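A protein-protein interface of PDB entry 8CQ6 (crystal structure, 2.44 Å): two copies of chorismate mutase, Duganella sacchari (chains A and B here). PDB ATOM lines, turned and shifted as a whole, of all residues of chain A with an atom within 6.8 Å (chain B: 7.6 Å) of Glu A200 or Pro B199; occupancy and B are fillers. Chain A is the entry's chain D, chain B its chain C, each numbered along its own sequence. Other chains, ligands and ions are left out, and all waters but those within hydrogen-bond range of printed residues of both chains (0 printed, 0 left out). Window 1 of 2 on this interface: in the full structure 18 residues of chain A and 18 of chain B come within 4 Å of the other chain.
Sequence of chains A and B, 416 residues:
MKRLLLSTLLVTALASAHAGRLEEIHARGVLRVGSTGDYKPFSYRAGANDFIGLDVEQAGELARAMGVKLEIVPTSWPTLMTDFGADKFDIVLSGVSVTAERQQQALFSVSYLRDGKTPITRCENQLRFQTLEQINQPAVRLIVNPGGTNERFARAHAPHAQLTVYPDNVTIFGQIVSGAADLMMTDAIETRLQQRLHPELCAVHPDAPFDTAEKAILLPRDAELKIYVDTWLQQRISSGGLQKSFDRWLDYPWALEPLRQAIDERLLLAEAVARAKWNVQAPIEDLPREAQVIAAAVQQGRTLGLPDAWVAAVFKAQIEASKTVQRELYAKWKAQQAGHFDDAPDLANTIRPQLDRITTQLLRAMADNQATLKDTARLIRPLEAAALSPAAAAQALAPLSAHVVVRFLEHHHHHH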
ATOM      1  N   THR A 121       2.035  18.287 -19.684  1.00  0.00           N
ATOM      2  CA  THR A 121       3.090  19.035 -20.346  1.00  0.00           C
ATOM      3  C   THR A 121       3.224  20.413 -19.699  1.00  0.00           C
ATOM      4  O   THR A 121       2.383  20.808 -18.894  1.00  0.00           O
ATOM      5  CB  THR A 121       2.819  19.149 -21.852  1.00  0.00           C
ATOM      6  OG1 THR A 121       4.000  19.628 -22.495  1.00  0.00           O
ATOM      7  CG2 THR A 121       1.659  20.064 -22.168  1.00  0.00           C
ATOM      8  N   ARG A 122       4.283  21.137 -20.077  1.00  0.00           N
ATOM      9  CA  ARG A 122       4.514  22.492 -19.604  1.00  0.00           C
ATOM     10  C   ARG A 122       3.360  23.391 -20.045  1.00  0.00           C
ATOM     11  O   ARG A 122       2.792  23.180 -21.115  1.00  0.00           O
ATOM     12  CB  ARG A 122       5.861  22.991 -20.135  1.00  0.00           C
ATOM     13  CG  ARG A 122       7.069  22.412 -19.412  1.00  0.00           C
ATOM     14  CD  ARG A 122       8.406  22.884 -19.952  1.00  0.00           C
ATOM     15  NE  ARG A 122       9.174  23.597 -18.938  1.00  0.00           N
ATOM     16  CZ  ARG A 122       8.843  24.773 -18.415  1.00  0.00           C
ATOM     17  NH1 ARG A 122       8.158  25.646 -19.129  1.00  0.00           N
ATOM     18  NH2 ARG A 122       9.200  25.068 -17.178  1.00  0.00           N
ATOM     19  N   CYS A 123       3.026  24.388 -19.210  1.00  0.00           N
ATOM     20  CA  CYS A 123       1.766  25.115 -19.299  1.00  0.00           C
ATOM     21  C   CYS A 123       1.686  25.921 -20.597  1.00  0.00           C
ATOM     22  O   CYS A 123       0.582  26.174 -21.084  1.00  0.00           O
ATOM     23  CB  CYS A 123       1.562  26.047 -18.105  1.00  0.00           C
ATOM     24  SG  CYS A 123       1.234  25.209 -16.525  1.00  0.00           S
ATOM     25  N   GLU A 124       2.847  26.317 -21.157  1.00  0.00           N
ATOM     26  CA  GLU A 124       2.922  26.884 -22.499  1.00  0.00           C
ATOM     27  C   GLU A 124       2.267  25.965 -23.527  1.00  0.00           C
ATOM     28  O   GLU A 124       1.431  26.402 -24.321  1.00  0.00           O
ATOM     29  CB  GLU A 124       4.371  27.026 -22.964  1.00  0.00           C
ATOM     30  CG  GLU A 124       5.197  27.957 -22.125  1.00  0.00           C
ATOM     31  CD  GLU A 124       6.418  27.322 -21.482  1.00  0.00           C
ATOM     32  OE1 GLU A 124       6.211  26.596 -20.516  1.00  0.00           O
ATOM     33  OE2 GLU A 124       7.567  27.583 -21.931  1.00  0.00           O
ATOM     34  N   ILE A 176      10.002  16.662 -17.747  1.00  0.00           N
ATOM     35  CA  ILE A 176       9.172  17.540 -18.559  1.00  0.00           C
ATOM     36  C   ILE A 176       9.439  18.988 -18.155  1.00  0.00           C
ATOM     37  O   ILE A 176       9.697  19.831 -19.017  1.00  0.00           O
ATOM     38  CB  ILE A 176       7.677  17.175 -18.433  1.00  0.00           C
ATOM     39  CG1 ILE A 176       7.418  15.715 -18.818  1.00  0.00           C
ATOM     40  CG2 ILE A 176       6.812  18.123 -19.245  1.00  0.00           C
ATOM     41  CD1 ILE A 176       6.186  15.116 -18.170  1.00  0.00           C
ATOM     42  N   VAL A 177       9.383  19.252 -16.843  1.00  0.00           N
ATOM     43  CA  VAL A 177       9.736  20.550 -16.284  1.00  0.00           C
ATOM     44  C   VAL A 177      11.026  21.050 -16.935  1.00  0.00           C
ATOM     45  O   VAL A 177      11.102  22.207 -17.337  1.00  0.00           O
ATOM     46  CB  VAL A 177       9.876  20.484 -14.749  1.00  0.00           C
ATOM     47  CG1 VAL A 177      10.593  21.701 -14.188  1.00  0.00           C
ATOM     48  CG2 VAL A 177       8.535  20.287 -14.070  1.00  0.00           C
ATOM     49  N   SER A 178      12.030  20.167 -17.031  1.00  0.00           N
ATOM     50  CA  SER A 178      13.373  20.571 -17.411  1.00  0.00           C
ATOM     51  C   SER A 178      13.570  20.480 -18.925  1.00  0.00           C
ATOM     52  O   SER A 178      14.696  20.602 -19.401  1.00  0.00           O
ATOM     53  CB  SER A 178      14.401  19.748 -16.676  1.00  0.00           C
ATOM     54  OG  SER A 178      14.497  18.442 -17.228  1.00  0.00           O
ATOM     55  N   GLN A 194       0.154  15.945 -10.278  1.00  0.00           N
ATOM     56  CA  GLN A 194       1.501  16.360 -10.635  1.00  0.00           C
ATOM     57  C   GLN A 194       1.522  17.824 -11.083  1.00  0.00           C
ATOM     58  O   GLN A 194       2.565  18.467 -11.030  1.00  0.00           O
ATOM     59  CB  GLN A 194       2.062  15.438 -11.713  1.00  0.00           C
ATOM     60  CG  GLN A 194       2.323  14.031 -11.202  1.00  0.00           C
ATOM     61  CD  GLN A 194       3.396  13.992 -10.145  1.00  0.00           C
ATOM     62  OE1 GLN A 194       4.260  14.861 -10.073  1.00  0.00           O
ATOM     63  NE2 GLN A 194       3.335  12.979  -9.300  1.00  0.00           N
ATOM     64  N   GLN A 195       0.367  18.352 -11.509  1.00  0.00           N
ATOM     65  CA  GLN A 195       0.265  19.757 -11.876  1.00  0.00           C
ATOM     66  C   GLN A 195       0.263  20.632 -10.619  1.00  0.00           C
ATOM     67  O   GLN A 195       0.678  21.788 -10.668  1.00  0.00           O
ATOM     68  CB  GLN A 195      -0.973  19.999 -12.751  1.00  0.00           C
ATOM     69  CG  GLN A 195      -2.182  20.562 -12.013  1.00  0.00           C
ATOM     70  CD  GLN A 195      -3.235  21.106 -12.946  1.00  0.00           C
ATOM     71  OE1 GLN A 195      -3.286  20.780 -14.126  1.00  0.00           O
ATOM     72  NE2 GLN A 195      -4.069  21.984 -12.416  1.00  0.00           N
ATOM     73  N   LEU A 197       1.998  19.590  -7.891  1.00  0.00           N
ATOM     74  CA  LEU A 197       3.332  19.410  -7.334  1.00  0.00           C
ATOM     75  C   LEU A 197       4.332  20.279  -8.090  1.00  0.00           C
ATOM     76  O   LEU A 197       5.147  20.966  -7.482  1.00  0.00           O
ATOM     77  CB  LEU A 197       3.755  17.936  -7.415  1.00  0.00           C
ATOM     78  CG  LEU A 197       3.008  16.933  -6.532  1.00  0.00           C
ATOM     79  CD1 LEU A 197       3.857  15.689  -6.287  1.00  0.00           C
ATOM     80  CD2 LEU A 197       2.598  17.533  -5.196  1.00  0.00           C
ATOM     81  N   HIS A 198       4.287  20.210  -9.424  1.00  0.00           N
ATOM     82  CA  HIS A 198       5.098  21.068 -10.274  1.00  0.00           C
ATOM     83  C   HIS A 198       4.222  22.182 -10.837  1.00  0.00           C
ATOM     84  O   HIS A 198       3.489  21.957 -11.793  1.00  0.00           O
ATOM     85  CB  HIS A 198       5.770  20.232 -11.374  1.00  0.00           C
ATOM     86  CG  HIS A 198       6.472  19.011 -10.862  1.00  0.00           C
ATOM     87  ND1 HIS A 198       7.647  19.121 -10.149  1.00  0.00           N
ATOM     88  CD2 HIS A 198       6.176  17.704 -10.884  1.00  0.00           C
ATOM     89  CE1 HIS A 198       8.048  17.915  -9.776  1.00  0.00           C
ATOM     90  NE2 HIS A 198       7.163  17.044 -10.203  1.00  0.00           N
ATOM     91  N   PRO A 199       4.258  23.419 -10.283  1.00  0.00           N
ATOM     92  CA  PRO A 199       3.400  24.503 -10.777  1.00  0.00           C
ATOM     93  C   PRO A 199       3.615  24.836 -12.255  1.00  0.00           C
ATOM     94  O   PRO A 199       2.722  25.376 -12.905  1.00  0.00           O
ATOM     95  CB  PRO A 199       3.786  25.704  -9.894  1.00  0.00           C
ATOM     96  CG  PRO A 199       5.157  25.352  -9.348  1.00  0.00           C
ATOM     97  CD  PRO A 199       5.111  23.851  -9.163  1.00  0.00           C
ATOM     98  N   GLU A 200       4.806  24.492 -12.768  1.00  0.00           N
ATOM     99  CA  GLU A 200       5.204  24.763 -14.140  1.00  0.00           C
ATOM    100  C   GLU A 200       4.560  23.763 -15.101  1.00  0.00           C
ATOM    101  O   GLU A 200       4.479  24.035 -16.297  1.00  0.00           O
ATOM    102  CB  GLU A 200       6.729  24.721 -14.273  1.00  0.00           C
ATOM    103  CG  GLU A 200       7.367  23.475 -13.669  1.00  0.00           C
ATOM    104  CD  GLU A 200       7.927  23.597 -12.255  1.00  0.00           C
ATOM    105  OE1 GLU A 200       7.140  23.583 -11.307  1.00  0.00           O
ATOM    106  OE2 GLU A 200       9.169  23.641 -12.116  1.00  0.00           O
ATOM    107  N   LEU A 201       4.112  22.612 -14.585  1.00  0.00           N
ATOM    108  CA  LEU A 201       3.374  21.638 -15.380  1.00  0.00           C
ATOM    109  C   LEU A 201       1.870  21.879 -15.262  1.00  0.00           C
ATOM    110  O   LEU A 201       1.384  22.391 -14.249  1.00  0.00           O
ATOM    111  CB  LEU A 201       3.717  20.222 -14.908  1.00  0.00           C
ATOM    112  CG  LEU A 201       5.136  19.744 -15.194  1.00  0.00           C
ATOM    113  CD1 LEU A 201       5.252  18.250 -14.942  1.00  0.00           C
ATOM    114  CD2 LEU A 201       5.560  20.065 -16.615  1.00  0.00           C
ATOM    115  N   CYS A 202       1.158  21.467 -16.321  1.00  0.00           N
ATOM    116  CA  CYS A 202      -0.279  21.640 -16.461  1.00  0.00           C
ATOM    117  C   CYS A 202      -0.879  20.369 -17.059  1.00  0.00           C
ATOM    118  O   CYS A 202      -0.324  19.774 -17.980  1.00  0.00           O
ATOM    119  CB  CYS A 202      -0.612  22.833 -17.352  1.00  0.00           C
ATOM    120  SG  CYS A 202      -0.696  24.443 -16.509  1.00  0.00           S
ATOM    121  N   THR B 121      -4.734  33.388 -12.756  1.00  0.00           N
ATOM    122  CA  THR B 121      -4.822  33.029 -11.351  1.00  0.00           C
ATOM    123  C   THR B 121      -3.834  31.899 -11.067  1.00  0.00           C
ATOM    124  O   THR B 121      -3.272  31.310 -11.991  1.00  0.00           O
ATOM    125  CB  THR B 121      -6.254  32.637 -10.964  1.00  0.00           C
ATOM    126  OG1 THR B 121      -6.335  32.577  -9.539  1.00  0.00           O
ATOM    127  CG2 THR B 121      -6.677  31.313 -11.560  1.00  0.00           C
ATOM    128  N   ARG B 122      -3.648  31.606  -9.775  1.00  0.00           N
ATOM    129  CA  ARG B 122      -2.790  30.516  -9.339  1.00  0.00           C
ATOM    130  C   ARG B 122      -3.327  29.192  -9.880  1.00  0.00           C
ATOM    131  O   ARG B 122      -4.539  29.029 -10.002  1.00  0.00           O
ATOM    132  CB  ARG B 122      -2.713  30.513  -7.809  1.00  0.00           C
ATOM    133  CG  ARG B 122      -1.809  31.597  -7.240  1.00  0.00           C
ATOM    134  CD  ARG B 122      -1.676  31.551  -5.726  1.00  0.00           C
ATOM    135  NE  ARG B 122      -0.302  31.320  -5.286  1.00  0.00           N
ATOM    136  CZ  ARG B 122       0.413  30.225  -5.539  1.00  0.00           C
ATOM    137  NH1 ARG B 122      -0.178  29.049  -5.647  1.00  0.00           N
ATOM    138  NH2 ARG B 122       1.726  30.312  -5.673  1.00  0.00           N
ATOM    139  N   CYS B 123      -2.411  28.258 -10.180  1.00  0.00           N
ATOM    140  CA  CYS B 123      -2.695  27.084 -10.997  1.00  0.00           C
ATOM    141  C   CYS B 123      -3.703  26.162 -10.305  1.00  0.00           C
ATOM    142  O   CYS B 123      -4.437  25.439 -10.979  1.00  0.00           O
ATOM    143  CB  CYS B 123      -1.403  26.329 -11.316  1.00  0.00           C
ATOM    144  SG  CYS B 123      -1.567  24.822 -12.314  1.00  0.00           S
ATOM    145  N   VAL B 177       0.473  35.671  -7.223  1.00  0.00           N
ATOM    146  CA  VAL B 177       1.428  34.689  -6.734  1.00  0.00           C
ATOM    147  C   VAL B 177       1.373  34.640  -5.206  1.00  0.00           C
ATOM    148  O   VAL B 177       1.332  33.560  -4.623  1.00  0.00           O
ATOM    149  CB  VAL B 177       2.856  34.986  -7.236  1.00  0.00           C
ATOM    150  CG1 VAL B 177       3.911  34.213  -6.453  1.00  0.00           C
ATOM    151  CG2 VAL B 177       2.996  34.736  -8.735  1.00  0.00           C
ATOM    152  N   GLN B 194       2.662  35.779 -18.933  1.00  0.00           N
ATOM    153  CA  GLN B 194       2.883  35.889 -17.501  1.00  0.00           C
ATOM    154  C   GLN B 194       2.856  34.512 -16.842  1.00  0.00           C
ATOM    155  O   GLN B 194       3.402  34.352 -15.757  1.00  0.00           O
ATOM    156  CB  GLN B 194       1.832  36.805 -16.867  1.00  0.00           C
ATOM    157  CG  GLN B 194       1.997  38.274 -17.214  1.00  0.00           C
ATOM    158  CD  GLN B 194       3.326  38.833 -16.766  1.00  0.00           C
ATOM    159  OE1 GLN B 194       3.911  38.388 -15.786  1.00  0.00           O
ATOM    160  NE2 GLN B 194       3.803  39.844 -17.470  1.00  0.00           N
ATOM    161  N   GLN B 195       2.230  33.522 -17.489  1.00  0.00           N
ATOM    162  CA  GLN B 195       2.221  32.161 -16.975  1.00  0.00           C
ATOM    163  C   GLN B 195       3.585  31.505 -17.191  1.00  0.00           C
ATOM    164  O   GLN B 195       3.965  30.623 -16.422  1.00  0.00           O
ATOM    165  CB  GLN B 195       1.074  31.354 -17.588  1.00  0.00           C
ATOM    166  CG  GLN B 195       1.489  30.426 -18.721  1.00  0.00           C
ATOM    167  CD  GLN B 195       0.305  29.742 -19.362  1.00  0.00           C
ATOM    168  OE1 GLN B 195      -0.759  29.589 -18.757  1.00  0.00           O
ATOM    169  NE2 GLN B 195       0.472  29.345 -20.615  1.00  0.00           N
ATOM    170  N   ARG B 196       4.301  31.927 -18.241  1.00  0.00           N
ATOM    171  CA  ARG B 196       5.687  31.527 -18.455  1.00  0.00           C
ATOM    172  C   ARG B 196       6.601  32.175 -17.415  1.00  0.00           C
ATOM    173  O   ARG B 196       7.501  31.522 -16.897  1.00  0.00           O
ATOM    174  CB  ARG B 196       6.152  31.894 -19.868  1.00  0.00           C
ATOM    175  CG  ARG B 196       5.818  30.850 -20.919  1.00  0.00           C
ATOM    176  CD  ARG B 196       6.642  31.030 -22.176  1.00  0.00           C
ATOM    177  NE  ARG B 196       6.410  32.336 -22.757  1.00  0.00           N
ATOM    178  CZ  ARG B 196       7.073  32.845 -23.787  1.00  0.00           C
ATOM    179  NH1 ARG B 196       8.297  32.445 -24.101  1.00  0.00           N
ATOM    180  NH2 ARG B 196       6.498  33.797 -24.495  1.00  0.00           N
ATOM    181  N   LEU B 197       6.374  33.459 -17.113  1.00  0.00           N
ATOM    182  CA  LEU B 197       7.263  34.219 -16.246  1.00  0.00           C
ATOM    183  C   LEU B 197       7.098  33.770 -14.794  1.00  0.00           C
ATOM    184  O   LEU B 197       8.087  33.546 -14.107  1.00  0.00           O
ATOM    185  CB  LEU B 197       6.972  35.718 -16.384  1.00  0.00           C
ATOM    186  CG  LEU B 197       7.337  36.361 -17.722  1.00  0.00           C
ATOM    187  CD1 LEU B 197       7.367  37.877 -17.588  1.00  0.00           C
ATOM    188  CD2 LEU B 197       8.670  35.842 -18.253  1.00  0.00           C
ATOM    189  N   HIS B 198       5.854  33.671 -14.327  1.00  0.00           N
ATOM    190  CA  HIS B 198       5.563  33.118 -13.016  1.00  0.00           C
ATOM    191  C   HIS B 198       5.040  31.689 -13.180  1.00  0.00           C
ATOM    192  O   HIS B 198       3.868  31.497 -13.503  1.00  0.00           O
ATOM    193  CB  HIS B 198       4.556  34.001 -12.267  1.00  0.00           C
ATOM    194  CG  HIS B 198       4.884  35.456 -12.264  1.00  0.00           C
ATOM    195  ND1 HIS B 198       4.832  36.255 -13.383  1.00  0.00           N
ATOM    196  CD2 HIS B 198       5.214  36.268 -11.256  1.00  0.00           C
ATOM    197  CE1 HIS B 198       5.127  37.504 -13.050  1.00  0.00           C
ATOM    198  NE2 HIS B 198       5.344  37.540 -11.755  1.00  0.00           N
ATOM    199  N   PRO B 199       5.868  30.634 -12.972  1.00  0.00           N
ATOM    200  CA  PRO B 199       5.405  29.252 -13.155  1.00  0.00           C
ATOM    201  C   PRO B 199       4.209  28.878 -12.276  1.00  0.00           C
ATOM    202  O   PRO B 199       3.452  27.965 -12.606  1.00  0.00           O
ATOM    203  CB  PRO B 199       6.633  28.403 -12.794  1.00  0.00           C
ATOM    204  CG  PRO B 199       7.495  29.328 -11.955  1.00  0.00           C
ATOM    205  CD  PRO B 199       7.275  30.701 -12.550  1.00  0.00           C
ATOM    206  N   GLU B 200       4.048  29.610 -11.164  1.00  0.00           N
ATOM    207  CA  GLU B 200       2.998  29.373 -10.184  1.00  0.00           C
ATOM    208  C   GLU B 200       1.656  29.920 -10.675  1.00  0.00           C
ATOM    209  O   GLU B 200       0.613  29.517 -10.168  1.00  0.00           O
ATOM    210  CB  GLU B 200       3.371  30.004  -8.840  1.00  0.00           C
ATOM    211  CG  GLU B 200       3.818  31.453  -8.941  1.00  0.00           C
ATOM    212  CD  GLU B 200       5.319  31.715  -8.980  1.00  0.00           C
ATOM    213  OE1 GLU B 200       5.921  31.508 -10.037  1.00  0.00           O
ATOM    214  OE2 GLU B 200       5.864  32.189  -7.952  1.00  0.00           O
ATOM    215  N   LEU B 201       1.685  30.847 -11.643  1.00  0.00           N
ATOM    216  CA  LEU B 201       0.472  31.358 -12.269  1.00  0.00           C
ATOM    217  C   LEU B 201       0.142  30.559 -13.531  1.00  0.00           C
ATOM    218  O   LEU B 201       1.038  30.014 -14.181  1.00  0.00           O
ATOM    219  CB  LEU B 201       0.655  32.841 -12.607  1.00  0.00           C
ATOM    220  CG  LEU B 201       0.738  33.796 -11.415  1.00  0.00           C
ATOM    221  CD1 LEU B 201       0.662  35.249 -11.878  1.00  0.00           C
ATOM    222  CD2 LEU B 201      -0.353  33.504 -10.391  1.00  0.00           C
ATOM    223  N   CYS B 202      -1.162  30.533 -13.855  1.00  0.00           N
ATOM    224  CA  CYS B 202      -1.716  29.797 -14.981  1.00  0.00           C
ATOM    225  C   CYS B 202      -2.770  30.659 -15.682  1.00  0.00           C
ATOM    226  O   CYS B 202      -3.592  31.310 -15.034  1.00  0.00           O
ATOM    227  CB  CYS B 202      -2.344  28.477 -14.535  1.00  0.00           C
ATOM    228  SG  CYS B 202      -1.187  27.082 -14.464  1.00  0.00           S
ATOM    229  N   ASP B 368      16.226  28.617 -12.564  1.00  0.00           N
ATOM    230  CA  ASP B 368      14.806  28.659 -12.889  1.00  0.00           C
ATOM    231  C   ASP B 368      14.597  28.165 -14.320  1.00  0.00           C
ATOM    232  O   ASP B 368      13.672  27.392 -14.568  1.00  0.00           O
ATOM    233  CB  ASP B 368      14.210  30.044 -12.617  1.00  0.00           C
ATOM    234  CG  ASP B 368      14.187  30.436 -11.143  1.00  0.00           C
ATOM    235  OD1 ASP B 368      14.519  29.588 -10.284  1.00  0.00           O
ATOM    236  OD2 ASP B 368      13.832  31.597 -10.857  1.00  0.00           O
ATOM    237  N   ASN B 369      15.446  28.607 -15.262  1.00  0.00           N
ATOM    238  CA  ASN B 369      15.118  28.579 -16.684  1.00  0.00           C
ATOM    239  C   ASN B 369      16.002  27.569 -17.411  1.00  0.00           C
ATOM    240  O   ASN B 369      16.664  27.900 -18.397  1.00  0.00           O
ATOM    241  CB  ASN B 369      15.298  29.949 -17.331  1.00  0.00           C
ATOM    242  CG  ASN B 369      14.688  31.060 -16.510  1.00  0.00           C
ATOM    243  OD1 ASN B 369      13.862  30.822 -15.634  1.00  0.00           O
ATOM    244  ND2 ASN B 369      15.060  32.297 -16.784  1.00  0.00           N
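The side-chain amide nitrogen of Gln B195 lies within hydrogen-bond range of the backbone carbonyl oxygen of Cys A123. SG of Cys B123 sits at hydrogen-bond distance from NE2 of Gln A195, at 3.8 Å. O of Pro B199 lies close to O of Pro A199 (2.7 Å). The side-chain sulfur of Cys B202 lies within hydrogen-bond range of the side-chain sulfur of Cys A202 (3.4 Å). The side-chain sulfur (SG) of Cys B202 is in hydrogen-bond range of the side-chain sulfur (SG) of Cys A123 (3.7 Å).
The backbone carbonyl oxygen of Glu B200 lies within hydrogen-bond range of the backbone NH of Cys B123 (3.3 Å). O of Glu A200 sits at hydrogen-bond distance from N of Cys A123. The side-chain sulfur (SG) of Cys A123 forms a disulfide with the side-chain sulfur (SG) of Cys A202. The side-chain carboxylate (OE1) of Glu A124 lies within salt-bridge range of the guanidinium group (NH1) of Arg A122 (2.6 Å). The backbone carbonyl oxygen (O) of Thr A121 is in hydrogen-bond range of the backbone NH (N) of Cys A202. The backbone NH of Cys B202 is in hydrogen-bond range of the backbone carbonyl oxygen of Thr B121 (2.9 Å).
Among the printed residues, pairs that only touch across the chains: Glu A124 with Gln B195 (3.9 Å), Glu A124 with Arg B196 (3.2 Å), Pro A199 with Glu B200 (3.8 Å) and Glu A200 with Pro B199 (3.7 Å).
Of the printed residues of chain B, Gln A195 touches Cys B123 (3.8 Å). Pro A199 touches just these residues of chain B: Pro B199 and Glu B200. Glu A200 touches just one residue of chain B: Pro B199 (3.7 Å). Of the printed residues of chain B, Cys A202 touches Cys B202. Printed residues of chain A within 4 Å of Arg B196: Glu A124. Leu B197 touches none of the printed residues of chain A. Of the printed residues of chain A, Glu B200 touches Pro A199 (3.8 Å). Printed residues of chain A within 4 Å of Cys B202: Cys A123 (3.7 Å) and Cys A202 (3.4 Å). The nearest residue of chain A that does not touch Pro B199 is Cys A123 (5.3 Å).
Along chain A the printed residues that touch a printed residue of chain B span positions 123 to 202. Printed residues of chain B that touch a printed residue of chain A: Cys B123, Gln B195, Arg B196, Pro B199, Glu B200 and Cys B202. Hydrophobic or aromatic side chains of chain B within 4 Å of the printed part of chain A: Pro B199. Among the printed residues, 9 pairs touch across the chains. Among the printed residues, no Asp or Glu carboxylate lies within 4 Å of a Lys or Arg side-chain nitrogen of the other chain.
Cys A123 touches Gln B195, and with the chains exchanged Gln A195 touches Cys B123. Cys A123 touches Cys B202, but with the chains exchanged Cys A202 does not touch Cys B123 (4.3 Å). Pro A199 touches its own counterpart, Pro B199. Cys A202 touches its own counterpart, Cys B202. Positions printed for both chains: 121, 122, 123, 177, 194, 195, 197, 198, 199, 200, 201 and 202. Of the 9 pairs that touch across the chains among the printed residues, 6 have their exchanged pair printed and touching as well.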
